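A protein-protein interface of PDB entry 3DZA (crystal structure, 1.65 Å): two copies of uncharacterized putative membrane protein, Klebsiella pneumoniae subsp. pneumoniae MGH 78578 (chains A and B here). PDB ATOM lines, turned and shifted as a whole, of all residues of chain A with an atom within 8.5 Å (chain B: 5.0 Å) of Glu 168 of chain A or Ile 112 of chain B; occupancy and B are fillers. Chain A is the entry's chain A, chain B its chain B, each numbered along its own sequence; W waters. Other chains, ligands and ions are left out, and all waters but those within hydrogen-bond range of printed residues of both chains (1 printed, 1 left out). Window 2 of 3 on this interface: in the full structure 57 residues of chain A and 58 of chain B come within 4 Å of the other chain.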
ATOM      1  N   ARG A  43     -24.628 -19.809   1.869  1.00  0.00           N
ATOM      2  CA  ARG A  43     -24.958 -20.906   1.006  1.00  0.00           C
ATOM      3  C   ARG A  43     -25.849 -21.947   1.745  1.00  0.00           C
ATOM      4  O   ARG A  43     -26.831 -22.475   1.184  1.00  0.00           O
ATOM      5  CB  ARG A  43     -23.688 -21.571   0.449  1.00  0.00           C
ATOM      6  CG  ARG A  43     -22.794 -20.668  -0.420  1.00  0.00           C
ATOM      7  CD  ARG A  43     -21.603 -21.428  -0.968  1.00  0.00           C
ATOM      8  NE  ARG A  43     -22.043 -22.506  -1.835  1.00  0.00           N
ATOM      9  CZ  ARG A  43     -21.501 -23.721  -1.917  1.00  0.00           C
ATOM     10  NH1 ARG A  43     -20.382 -24.020  -1.248  1.00  0.00           N
ATOM     11  NH2 ARG A  43     -22.029 -24.617  -2.760  1.00  0.00           N
ATOM     12  N   LEU A  46     -29.439 -20.557   1.997  1.00  0.00           N
ATOM     13  CA  LEU A  46     -30.186 -20.628   0.737  1.00  0.00           C
ATOM     14  C   LEU A  46     -30.871 -21.988   0.579  1.00  0.00           C
ATOM     15  O   LEU A  46     -32.062 -22.059   0.229  1.00  0.00           O
ATOM     16  CB  LEU A  46     -29.264 -20.360  -0.444  1.00  0.00           C
ATOM     17  CG  LEU A  46     -28.828 -18.923  -0.648  1.00  0.00           C
ATOM     18  CD1 LEU A  46     -27.843 -18.853  -1.786  1.00  0.00           C
ATOM     19  CD2 LEU A  46     -30.059 -17.975  -0.827  1.00  0.00           C
ATOM     20  N   PHE A  47     -30.129 -23.046   0.856  1.00  0.00           N
ATOM     21  CA  PHE A  47     -30.635 -24.400   0.665  1.00  0.00           C
ATOM     22  C   PHE A  47     -31.506 -24.882   1.797  1.00  0.00           C
ATOM     23  O   PHE A  47     -31.975 -26.028   1.768  1.00  0.00           O
ATOM     24  CB  PHE A  47     -29.502 -25.369   0.398  1.00  0.00           C
ATOM     25  CG  PHE A  47     -28.897 -25.202  -0.970  1.00  0.00           C
ATOM     26  CD1 PHE A  47     -29.639 -25.488  -2.113  1.00  0.00           C
ATOM     27  CD2 PHE A  47     -27.601 -24.750  -1.125  1.00  0.00           C
ATOM     28  CE1 PHE A  47     -29.096 -25.313  -3.387  1.00  0.00           C
ATOM     29  CE2 PHE A  47     -27.036 -24.594  -2.385  1.00  0.00           C
ATOM     30  CZ  PHE A  47     -27.790 -24.875  -3.529  1.00  0.00           C
ATOM     31  N   ALA A 153     -17.017 -10.939  -6.031  1.00  0.00           N
ATOM     32  CA  ALA A 153     -17.905 -12.122  -5.968  1.00  0.00           C
ATOM     33  C   ALA A 153     -19.074 -11.867  -5.003  1.00  0.00           C
ATOM     34  O   ALA A 153     -20.231 -12.228  -5.274  1.00  0.00           O
ATOM     35  CB  ALA A 153     -17.108 -13.369  -5.493  1.00  0.00           C
ATOM     36  N   GLN A 156     -21.560  -9.477  -6.534  1.00  0.00           N
ATOM     37  CA  GLN A 156     -22.268 -10.161  -7.578  1.00  0.00           C
ATOM     38  C   GLN A 156     -23.350 -11.056  -6.966  1.00  0.00           C
ATOM     39  O   GLN A 156     -24.474 -11.121  -7.470  1.00  0.00           O
ATOM     40  CB  GLN A 156     -21.260 -10.988  -8.374  1.00  0.00           C
ATOM     41  CG  GLN A 156     -21.805 -11.766  -9.518  1.00  0.00           C
ATOM     42  CD  GLN A 156     -20.703 -12.504 -10.286  1.00  0.00           C
ATOM     43  OE1 GLN A 156     -19.527 -12.491  -9.871  1.00  0.00           O
ATOM     44  NE2 GLN A 156     -21.068 -13.118 -11.411  1.00  0.00           N
ATOM     45  N   SER A 157     -23.019 -11.712  -5.854  1.00  0.00           N
ATOM     46  CA  SER A 157     -23.971 -12.564  -5.155  1.00  0.00           C
ATOM     47  C   SER A 157     -25.136 -11.722  -4.577  1.00  0.00           C
ATOM     48  O   SER A 157     -26.296 -12.139  -4.616  1.00  0.00           O
ATOM     49  CB  SER A 157     -23.270 -13.382  -4.066  1.00  0.00           C
ATOM     50  OG  SER A 157     -22.194 -14.142  -4.612  1.00  0.00           O
ATOM     51  N   LEU A 160     -27.514 -11.041  -7.482  1.00  0.00           N
ATOM     52  CA  LEU A 160     -28.279 -12.251  -7.821  1.00  0.00           C
ATOM     53  C   LEU A 160     -29.371 -12.545  -6.764  1.00  0.00           C
ATOM     54  O   LEU A 160     -30.485 -12.947  -7.114  1.00  0.00           O
ATOM     55  CB  LEU A 160     -27.310 -13.419  -7.975  1.00  0.00           C
ATOM     56  CG  LEU A 160     -26.515 -13.412  -9.276  1.00  0.00           C
ATOM     57  CD1 LEU A 160     -25.326 -14.389  -9.093  1.00  0.00           C
ATOM     58  CD2 LEU A 160     -27.326 -13.744 -10.544  1.00  0.00           C
ATOM     59  N   LEU A 161     -29.051 -12.403  -5.484  1.00  0.00           N
ATOM     60  CA  LEU A 161     -30.030 -12.645  -4.408  1.00  0.00           C
ATOM     61  C   LEU A 161     -31.209 -11.689  -4.572  1.00  0.00           C
ATOM     62  O   LEU A 161     -32.355 -12.091  -4.430  1.00  0.00           O
ATOM     63  CB  LEU A 161     -29.423 -12.515  -3.014  1.00  0.00           C
ATOM     64  CG  LEU A 161     -28.404 -13.606  -2.639  1.00  0.00           C
ATOM     65  CD1 LEU A 161     -27.760 -13.230  -1.279  1.00  0.00           C
ATOM     66  CD2 LEU A 161     -29.061 -14.987  -2.601  1.00  0.00           C
ATOM     67  N   ALA A 163     -32.344 -10.392  -7.255  1.00  0.00           N
ATOM     68  CA  ALA A 163     -33.075 -10.905  -8.410  1.00  0.00           C
ATOM     69  C   ALA A 163     -33.767 -12.262  -8.176  1.00  0.00           C
ATOM     70  O   ALA A 163     -34.437 -12.776  -9.077  1.00  0.00           O
ATOM     71  CB  ALA A 163     -32.119 -11.020  -9.586  1.00  0.00           C
ATOM     72  N   GLY A 164     -33.603 -12.848  -6.990  1.00  0.00           N
ATOM     73  CA  GLY A 164     -34.184 -14.118  -6.644  1.00  0.00           C
ATOM     74  C   GLY A 164     -33.507 -15.327  -7.281  1.00  0.00           C
ATOM     75  O   GLY A 164     -34.078 -16.441  -7.299  1.00  0.00           O
ATOM     76  N   LYS A 165     -32.283 -15.105  -7.771  1.00  0.00           N
ATOM     77  CA  LYS A 165     -31.485 -16.152  -8.417  1.00  0.00           C
ATOM     78  C   LYS A 165     -30.593 -16.842  -7.392  1.00  0.00           C
ATOM     79  O   LYS A 165     -29.349 -16.693  -7.394  1.00  0.00           O
ATOM     80  CB  LYS A 165     -30.697 -15.567  -9.567  1.00  0.00           C
ATOM     81  CG  LYS A 165     -31.592 -15.095 -10.708  1.00  0.00           C
ATOM     82  CD  LYS A 165     -30.766 -14.647 -11.879  1.00  0.00           C
ATOM     83  CE  LYS A 165     -31.626 -14.247 -13.075  1.00  0.00           C
ATOM     84  NZ  LYS A 165     -30.775 -13.717 -14.186  1.00  0.00           N
ATOM     85  N   TYR A 166     -31.253 -17.598  -6.509  1.00  0.00           N
ATOM     86  CA  TYR A 166     -30.624 -18.197  -5.328  1.00  0.00           C
ATOM     87  C   TYR A 166     -29.608 -19.272  -5.691  1.00  0.00           C
ATOM     88  O   TYR A 166     -28.489 -19.253  -5.164  1.00  0.00           O
ATOM     89  CB  TYR A 166     -31.680 -18.772  -4.394  1.00  0.00           C
ATOM     90  CG  TYR A 166     -32.708 -17.740  -3.963  1.00  0.00           C
ATOM     91  CD1 TYR A 166     -32.309 -16.563  -3.386  1.00  0.00           C
ATOM     92  CD2 TYR A 166     -34.054 -17.954  -4.151  1.00  0.00           C
ATOM     93  CE1 TYR A 166     -33.224 -15.600  -2.988  1.00  0.00           C
ATOM     94  CE2 TYR A 166     -34.979 -17.006  -3.750  1.00  0.00           C
ATOM     95  CZ  TYR A 166     -34.556 -15.833  -3.179  1.00  0.00           C
ATOM     96  OH  TYR A 166     -35.448 -14.858  -2.760  1.00  0.00           O
ATOM     97  N   TYR A 167     -29.970 -20.176  -6.592  1.00  0.00           N
ATOM     98  CA  TYR A 167     -28.994 -21.227  -7.001  1.00  0.00           C
ATOM     99  C   TYR A 167     -27.699 -20.603  -7.580  1.00  0.00           C
ATOM    100  O   TYR A 167     -26.559 -20.936  -7.207  1.00  0.00           O
ATOM    101  CB  TYR A 167     -29.642 -22.215  -7.980  1.00  0.00           C
ATOM    102  CG  TYR A 167     -28.671 -23.300  -8.310  1.00  0.00           C
ATOM    103  CD1 TYR A 167     -28.411 -24.290  -7.375  1.00  0.00           C
ATOM    104  CD2 TYR A 167     -27.937 -23.285  -9.481  1.00  0.00           C
ATOM    105  CE1 TYR A 167     -27.423 -25.313  -7.613  1.00  0.00           C
ATOM    106  CE2 TYR A 167     -26.987 -24.270  -9.745  1.00  0.00           C
ATOM    107  CZ  TYR A 167     -26.731 -25.286  -8.826  1.00  0.00           C
ATOM    108  OH  TYR A 167     -25.770 -26.251  -9.095  1.00  0.00           O
ATOM    109  N   GLU A 168     -27.855 -19.661  -8.488  1.00  0.00           N
ATOM    110  CA  GLU A 168     -26.730 -18.930  -9.095  1.00  0.00           C
ATOM    111  C   GLU A 168     -25.876 -18.155  -8.058  1.00  0.00           C
ATOM    112  O   GLU A 168     -24.637 -18.176  -8.094  1.00  0.00           O
ATOM    113  CB  GLU A 168     -27.263 -17.990 -10.206  1.00  0.00           C
ATOM    114  CG  GLU A 168     -28.033 -18.717 -11.332  1.00  0.00           C
ATOM    115  CD  GLU A 168     -29.571 -18.818 -11.137  1.00  0.00           C
ATOM    116  OE1 GLU A 168     -30.061 -18.862  -9.996  1.00  0.00           O
ATOM    117  OE2 GLU A 168     -30.276 -18.856 -12.174  1.00  0.00           O
ATOM    118  N   ALA A 169     -26.539 -17.469  -7.141  1.00  0.00           N
ATOM    119  CA  ALA A 169     -25.836 -16.776  -6.069  1.00  0.00           C
ATOM    120  C   ALA A 169     -25.008 -17.802  -5.265  1.00  0.00           C
ATOM    121  O   ALA A 169     -23.829 -17.570  -4.951  1.00  0.00           O
ATOM    122  CB  ALA A 169     -26.850 -16.025  -5.145  1.00  0.00           C
ATOM    123  N   ASN A 170     -25.612 -18.952  -4.962  1.00  0.00           N
ATOM    124  CA  ASN A 170     -24.886 -20.032  -4.325  1.00  0.00           C
ATOM    125  C   ASN A 170     -23.594 -20.388  -5.071  1.00  0.00           C
ATOM    126  O   ASN A 170     -22.543 -20.569  -4.429  1.00  0.00           O
ATOM    127  CB  ASN A 170     -25.786 -21.242  -4.132  1.00  0.00           C
ATOM    128  CG  ASN A 170     -25.129 -22.572  -4.502  1.00  0.00           C
ATOM    129  OD1 ASN A 170     -24.293 -23.099  -3.753  1.00  0.00           O
ATOM    130  ND2 ASN A 170     -25.567 -23.161  -5.641  1.00  0.00           N
ATOM    131  N   LEU A 171     -23.648 -20.533  -6.404  1.00  0.00           N
ATOM    132  CA  LEU A 171     -22.453 -20.925  -7.172  1.00  0.00           C
ATOM    133  C   LEU A 171     -21.384 -19.816  -7.223  1.00  0.00           C
ATOM    134  O   LEU A 171     -20.181 -20.091  -7.223  1.00  0.00           O
ATOM    135  CB  LEU A 171     -22.809 -21.394  -8.599  1.00  0.00           C
ATOM    136  CG  LEU A 171     -23.500 -22.753  -8.726  1.00  0.00           C
ATOM    137  CD1 LEU A 171     -23.676 -23.125 -10.202  1.00  0.00           C
ATOM    138  CD2 LEU A 171     -22.717 -23.895  -8.018  1.00  0.00           C
ATOM    139  N   VAL A 172     -21.814 -18.557  -7.269  1.00  0.00           N
ATOM    140  CA  VAL A 172     -20.861 -17.436  -7.179  1.00  0.00           C
ATOM    141  C   VAL A 172     -20.113 -17.475  -5.855  1.00  0.00           C
ATOM    142  O   VAL A 172     -18.902 -17.311  -5.809  1.00  0.00           O
ATOM    143  CB  VAL A 172     -21.534 -16.068  -7.406  1.00  0.00           C
ATOM    144  CG1 VAL A 172     -20.544 -14.939  -7.226  1.00  0.00           C
ATOM    145  CG2 VAL A 172     -22.174 -16.032  -8.836  1.00  0.00           C
ATOM    146  N   LEU A 173     -20.858 -17.703  -4.779  1.00  0.00           N
ATOM    147  CA  LEU A 173     -20.291 -17.823  -3.441  1.00  0.00           C
ATOM    148  C   LEU A 173     -19.377 -19.056  -3.348  1.00  0.00           C
ATOM    149  O   LEU A 173     -18.305 -19.007  -2.736  1.00  0.00           O
ATOM    150  CB  LEU A 173     -21.400 -17.904  -2.421  1.00  0.00           C
ATOM    151  CG  LEU A 173     -22.197 -16.605  -2.271  1.00  0.00           C
ATOM    152  CD1 LEU A 173     -23.371 -16.815  -1.337  1.00  0.00           C
ATOM    153  CD2 LEU A 173     -21.332 -15.396  -1.802  1.00  0.00           C
ATOM    154  N   LYS A 174     -19.794 -20.141  -3.974  1.00  0.00           N
ATOM    155  CA  LYS A 174     -18.956 -21.334  -4.072  1.00  0.00           C
ATOM    156  C   LYS A 174     -17.623 -21.004  -4.744  1.00  0.00           C
ATOM    157  O   LYS A 174     -16.562 -21.320  -4.221  1.00  0.00           O
ATOM    158  CB  LYS A 174     -19.676 -22.436  -4.845  1.00  0.00           C
ATOM    159  CG  LYS A 174     -18.941 -23.736  -4.912  1.00  0.00           C
ATOM    160  CD  LYS A 174     -19.806 -24.804  -5.597  1.00  0.00           C
ATOM    161  CE  LYS A 174     -19.098 -26.130  -5.735  1.00  0.00           C
ATOM    162  NZ  LYS A 174     -18.186 -26.176  -6.941  1.00  0.00           N
ATOM    163  N   GLY A 175     -17.684 -20.329  -5.883  1.00  0.00           N
ATOM    164  CA  GLY A 175     -16.481 -19.847  -6.553  1.00  0.00           C
ATOM    165  C   GLY A 175     -15.626 -18.970  -5.624  1.00  0.00           C
ATOM    166  O   GLY A 175     -14.392 -19.059  -5.613  1.00  0.00           O
ATOM    167  N   LYS B 108     -32.196 -28.256 -17.296  1.00  0.00           N
ATOM    168  CA  LYS B 108     -31.564 -27.796 -16.058  1.00  0.00           C
ATOM    169  C   LYS B 108     -31.918 -26.339 -15.749  1.00  0.00           C
ATOM    170  O   LYS B 108     -32.169 -25.968 -14.574  1.00  0.00           O
ATOM    171  CB  LYS B 108     -30.040 -27.996 -16.091  1.00  0.00           C
ATOM    172  CG  LYS B 108     -29.388 -27.760 -14.753  1.00  0.00           C
ATOM    173  CD  LYS B 108     -27.856 -27.628 -14.875  1.00  0.00           C
ATOM    174  CE  LYS B 108     -27.197 -28.963 -15.167  1.00  0.00           C
ATOM    175  NZ  LYS B 108     -25.712 -28.851 -15.133  1.00  0.00           N
ATOM    176  N   GLU B 109     -31.928 -25.493 -16.787  1.00  0.00           N
ATOM    177  CA  GLU B 109     -32.260 -24.078 -16.593  1.00  0.00           C
ATOM    178  C   GLU B 109     -33.655 -23.943 -16.026  1.00  0.00           C
ATOM    179  O   GLU B 109     -33.881 -23.170 -15.115  1.00  0.00           O
ATOM    180  CB  GLU B 109     -32.135 -23.305 -17.908  1.00  0.00           C
ATOM    181  CG  GLU B 109     -30.698 -23.116 -18.324  1.00  0.00           C
ATOM    182  CD  GLU B 109     -30.511 -22.688 -19.786  1.00  0.00           C
ATOM    183  OE1 GLU B 109     -31.473 -22.841 -20.553  1.00  0.00           O
ATOM    184  OE2 GLU B 109     -29.399 -22.220 -20.145  1.00  0.00           O
ATOM    185  N   SER B 110     -34.591 -24.723 -16.566  1.00  0.00           N
ATOM    186  CA  SER B 110     -35.971 -24.727 -16.077  1.00  0.00           C
ATOM    187  C   SER B 110     -36.047 -25.201 -14.625  1.00  0.00           C
ATOM    188  O   SER B 110     -36.788 -24.624 -13.783  1.00  0.00           O
ATOM    189  CB  SER B 110     -36.844 -25.609 -16.989  1.00  0.00           C
ATOM    190  OG  SER B 110     -37.124 -24.946 -18.210  1.00  0.00           O
ATOM    191  N   ALA B 111     -35.305 -26.259 -14.317  1.00  0.00           N
ATOM    192  CA  ALA B 111     -35.289 -26.814 -12.969  1.00  0.00           C
ATOM    193  C   ALA B 111     -34.713 -25.827 -11.982  1.00  0.00           C
ATOM    194  O   ALA B 111     -35.237 -25.679 -10.871  1.00  0.00           O
ATOM    195  CB  ALA B 111     -34.504 -28.098 -12.924  1.00  0.00           C
ATOM    196  N   ILE B 112     -33.633 -25.149 -12.385  1.00  0.00           N
ATOM    197  CA  ILE B 112     -33.032 -24.109 -11.527  1.00  0.00           C
ATOM    198  C   ILE B 112     -34.034 -22.973 -11.245  1.00  0.00           C
ATOM    199  O   ILE B 112     -34.182 -22.500 -10.101  1.00  0.00           O
ATOM    200  CB  ILE B 112     -31.702 -23.577 -12.099  1.00  0.00           C
ATOM    201  CG1 ILE B 112     -30.645 -24.670 -12.016  1.00  0.00           C
ATOM    202  CG2 ILE B 112     -31.230 -22.361 -11.331  1.00  0.00           C
ATOM    203  CD1 ILE B 112     -29.432 -24.402 -12.851  1.00  0.00           C
ATOM    204  N   GLN B 113     -34.761 -22.556 -12.268  1.00  0.00           N
ATOM    205  CA  GLN B 113     -35.722 -21.471 -12.113  1.00  0.00           C
ATOM    206  C   GLN B 113     -36.820 -21.915 -11.158  1.00  0.00           C
ATOM    207  O   GLN B 113     -37.241 -21.170 -10.278  1.00  0.00           O
ATOM    208  CB  GLN B 113     -36.283 -21.114 -13.481  1.00  0.00           C
ATOM    209  CG  GLN B 113     -37.256 -19.959 -13.537  1.00  0.00           C
ATOM    210  CD  GLN B 113     -37.560 -19.524 -15.002  1.00  0.00           C
ATOM    211  OE1 GLN B 113     -36.946 -20.020 -15.987  1.00  0.00           O
ATOM    212  NE2 GLN B 113     -38.522 -18.601 -15.146  1.00  0.00           N
ATOM    213  N   SER B 114     -37.259 -23.152 -11.328  1.00  0.00           N
ATOM    214  CA  SER B 114     -38.311 -23.712 -10.480  1.00  0.00           C
ATOM    215  C   SER B 114     -37.826 -23.852  -9.037  1.00  0.00           C
ATOM    216  O   SER B 114     -38.515 -23.460  -8.113  1.00  0.00           O
ATOM    217  CB  SER B 114     -38.779 -25.049 -11.027  1.00  0.00           C
ATOM    218  OG  SER B 114     -39.726 -25.591 -10.151  1.00  0.00           O
ATOM    219  N   ALA B 115     -36.606 -24.347  -8.855  1.00  0.00           N
ATOM    220  CA  ALA B 115     -36.009 -24.425  -7.514  1.00  0.00           C
ATOM    221  C   ALA B 115     -35.908 -23.065  -6.824  1.00  0.00           C
ATOM    222  O   ALA B 115     -36.224 -22.931  -5.630  1.00  0.00           O
ATOM    223  CB  ALA B 115     -34.665 -25.125  -7.574  1.00  0.00           C
ATOM    224  N   ASN B 116     -35.508 -22.051  -7.573  1.00  0.00           N
ATOM    225  CA  ASN B 116     -35.402 -20.691  -7.046  1.00  0.00           C
ATOM    226  C   ASN B 116     -36.733 -20.176  -6.560  1.00  0.00           C
ATOM    227  O   ASN B 116     -36.791 -19.568  -5.506  1.00  0.00           O
ATOM    228  CB  ASN B 116     -34.829 -19.740  -8.085  1.00  0.00           C
ATOM    229  CG  ASN B 116     -33.329 -19.904  -8.268  1.00  0.00           C
ATOM    230  OD1 ASN B 116     -32.612 -20.390  -7.358  1.00  0.00           O
ATOM    231  ND2 ASN B 116     -32.846 -19.452  -9.433  1.00  0.00           N
ATOM    232  N   GLU B 117     -37.776 -20.414  -7.357  1.00  0.00           N
ATOM    233  CA  GLU B 117     -39.136 -19.998  -6.999  1.00  0.00           C
ATOM    234  C   GLU B 117     -39.582 -20.689  -5.709  1.00  0.00           C
ATOM    235  O   GLU B 117     -40.186 -20.060  -4.832  1.00  0.00           O
ATOM    236  CB  GLU B 117     -40.115 -20.335  -8.135  1.00  0.00           C
ATOM    237  CG  GLU B 117     -39.870 -19.532  -9.375  1.00  0.00           C
ATOM    238  CD  GLU B 117     -40.593 -20.051 -10.645  1.00  0.00           C
ATOM    239  OE1 GLU B 117     -41.238 -21.136 -10.583  1.00  0.00           O
ATOM    240  OE2 GLU B 117     -40.495 -19.356 -11.709  1.00  0.00           O
ATOM    241  N   LEU B 131     -33.961 -29.852  -7.997  1.00  0.00           N
ATOM    242  CA  LEU B 131     -32.556 -29.870  -8.414  1.00  0.00           C
ATOM    243  C   LEU B 131     -32.028 -31.298  -8.592  1.00  0.00           C
ATOM    244  O   LEU B 131     -31.356 -31.592  -9.580  1.00  0.00           O
ATOM    245  CB  LEU B 131     -31.708 -29.152  -7.370  1.00  0.00           C
ATOM    246  CG  LEU B 131     -32.021 -27.650  -7.248  1.00  0.00           C
ATOM    247  CD1 LEU B 131     -31.286 -27.046  -6.065  1.00  0.00           C
ATOM    248  CD2 LEU B 131     -31.638 -26.924  -8.539  1.00  0.00           C
ATOM    249  N   ILE B 136     -28.586 -32.107 -10.231  1.00  0.00           N
ATOM    250  CA  ILE B 136     -27.877 -31.229  -9.332  1.00  0.00           C
ATOM    251  C   ILE B 136     -28.021 -31.730  -7.903  1.00  0.00           C
ATOM    252  O   ILE B 136     -29.114 -31.631  -7.339  1.00  0.00           O
ATOM    253  CB  ILE B 136     -28.406 -29.785  -9.436  1.00  0.00           C
ATOM    254  CG1 ILE B 136     -28.223 -29.264 -10.868  1.00  0.00           C
ATOM    255  CG2 ILE B 136     -27.758 -28.869  -8.404  1.00  0.00           C
ATOM    256  CD1 ILE B 136     -28.941 -27.890 -11.164  1.00  0.00           C
HETATM  257  O   HOH W   1     -32.901 -19.047 -12.792  1.00  0.00           O
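No position is printed for both chains.
Of the 9 pairs that touch across the chains among the printed residues, none has its exchanged pair printed and touching as well.
The backbone NH of Lys 165 of chain A is in hydrogen-bond range of the backbone carbonyl oxygen of Leu 160 of chain A, at 2.9 Å.
O of Tyr 167 of chain A lies within hydrogen-bond range of ND2 of Asn 170 of chain A, at 2.9 Å.
The side-chain amide nitrogen (ND2) of Asn 116 of chain B lies close to the backbone carbonyl oxygen (O) of Ile 112 of chain B, at 3.4 Å.
N of Ile 136 of chain B sits at hydrogen-bond distance from O of Leu 131 of chain B (2.9 Å).
The side-chain amide oxygen (OD1) of Asn 116 of chain B sits at hydrogen-bond distance from the backbone NH (N) of Tyr 166 of chain A (3.2 Å).
The backbone NH of Tyr 167 of chain A is in hydrogen-bond range of the side-chain amide oxygen of Asn 116 of chain B (2.8 Å).
ND2 of Asn 116 of chain B is in hydrogen-bond range of OE1 of Glu 168 of chain A (2.9 Å).
Among the printed residues, pairs that only touch across the chains: Phe 47 of chain A with Leu 131 of chain B, Gly 164 of chain A with Asn 116 of chain B, Lys 165 of chain A with Asn 116 of chain B, Tyr 167 of chain A with Ile 112 of chain B, Tyr 167 of chain A with Ile 136 of chain B and Glu 168 of chain A with Ile 112 of chain B.
Of the 12 printed residues of chain B, 4 touch a printed residue of chain A.
Hydrophobic or aromatic side chains of chain B that line the printed part of chain A: Ile 112, Leu 131 and Ile 136.
Of the 21 printed residues of chain A, 6 touch a printed residue of chain B.
Printed residues of chain A that touch a printed residue of chain B: Phe 47, Gly 164, Lys 165, Tyr 166, Tyr 167 and Glu 168.
Hydrophobic or aromatic side chains of chain A that line the printed part of chain B: Phe 47, Tyr 166 and Tyr 167.
Water W1 lies within hydrogen-bond range of the side-chain carboxylate of Glu 168 of chain A (2.7 Å) and the side-chain amide nitrogen of Asn 116 of chain B (3.4 Å).
Of the printed residues of chain B, Gly 164 of chain A touches Asn 116 (3.5 Å).
Glu 168 of chain A touches just these residues of chain B: Ile 112 and Asn 116.
No residue of chain A comes within 4 Å of Ala 111 of chain B.
Ile 112 of chain B touches two residues of chain A.
Of the printed residues of chain A, Ile 136 of chain B touches Tyr 167.
The nearest printed residue of chain B that does not touch Glu 168 of chain A is Gln 113 of chain B (5.8 Å).
The nearest residue of chain A that does not touch Ile 112 of chain B is Leu 171 of chain A (6.5 Å).
The nearest printed residue of chain A that does not touch Asn 116 of chain B is Ala 169 of chain A (6.7 Å).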
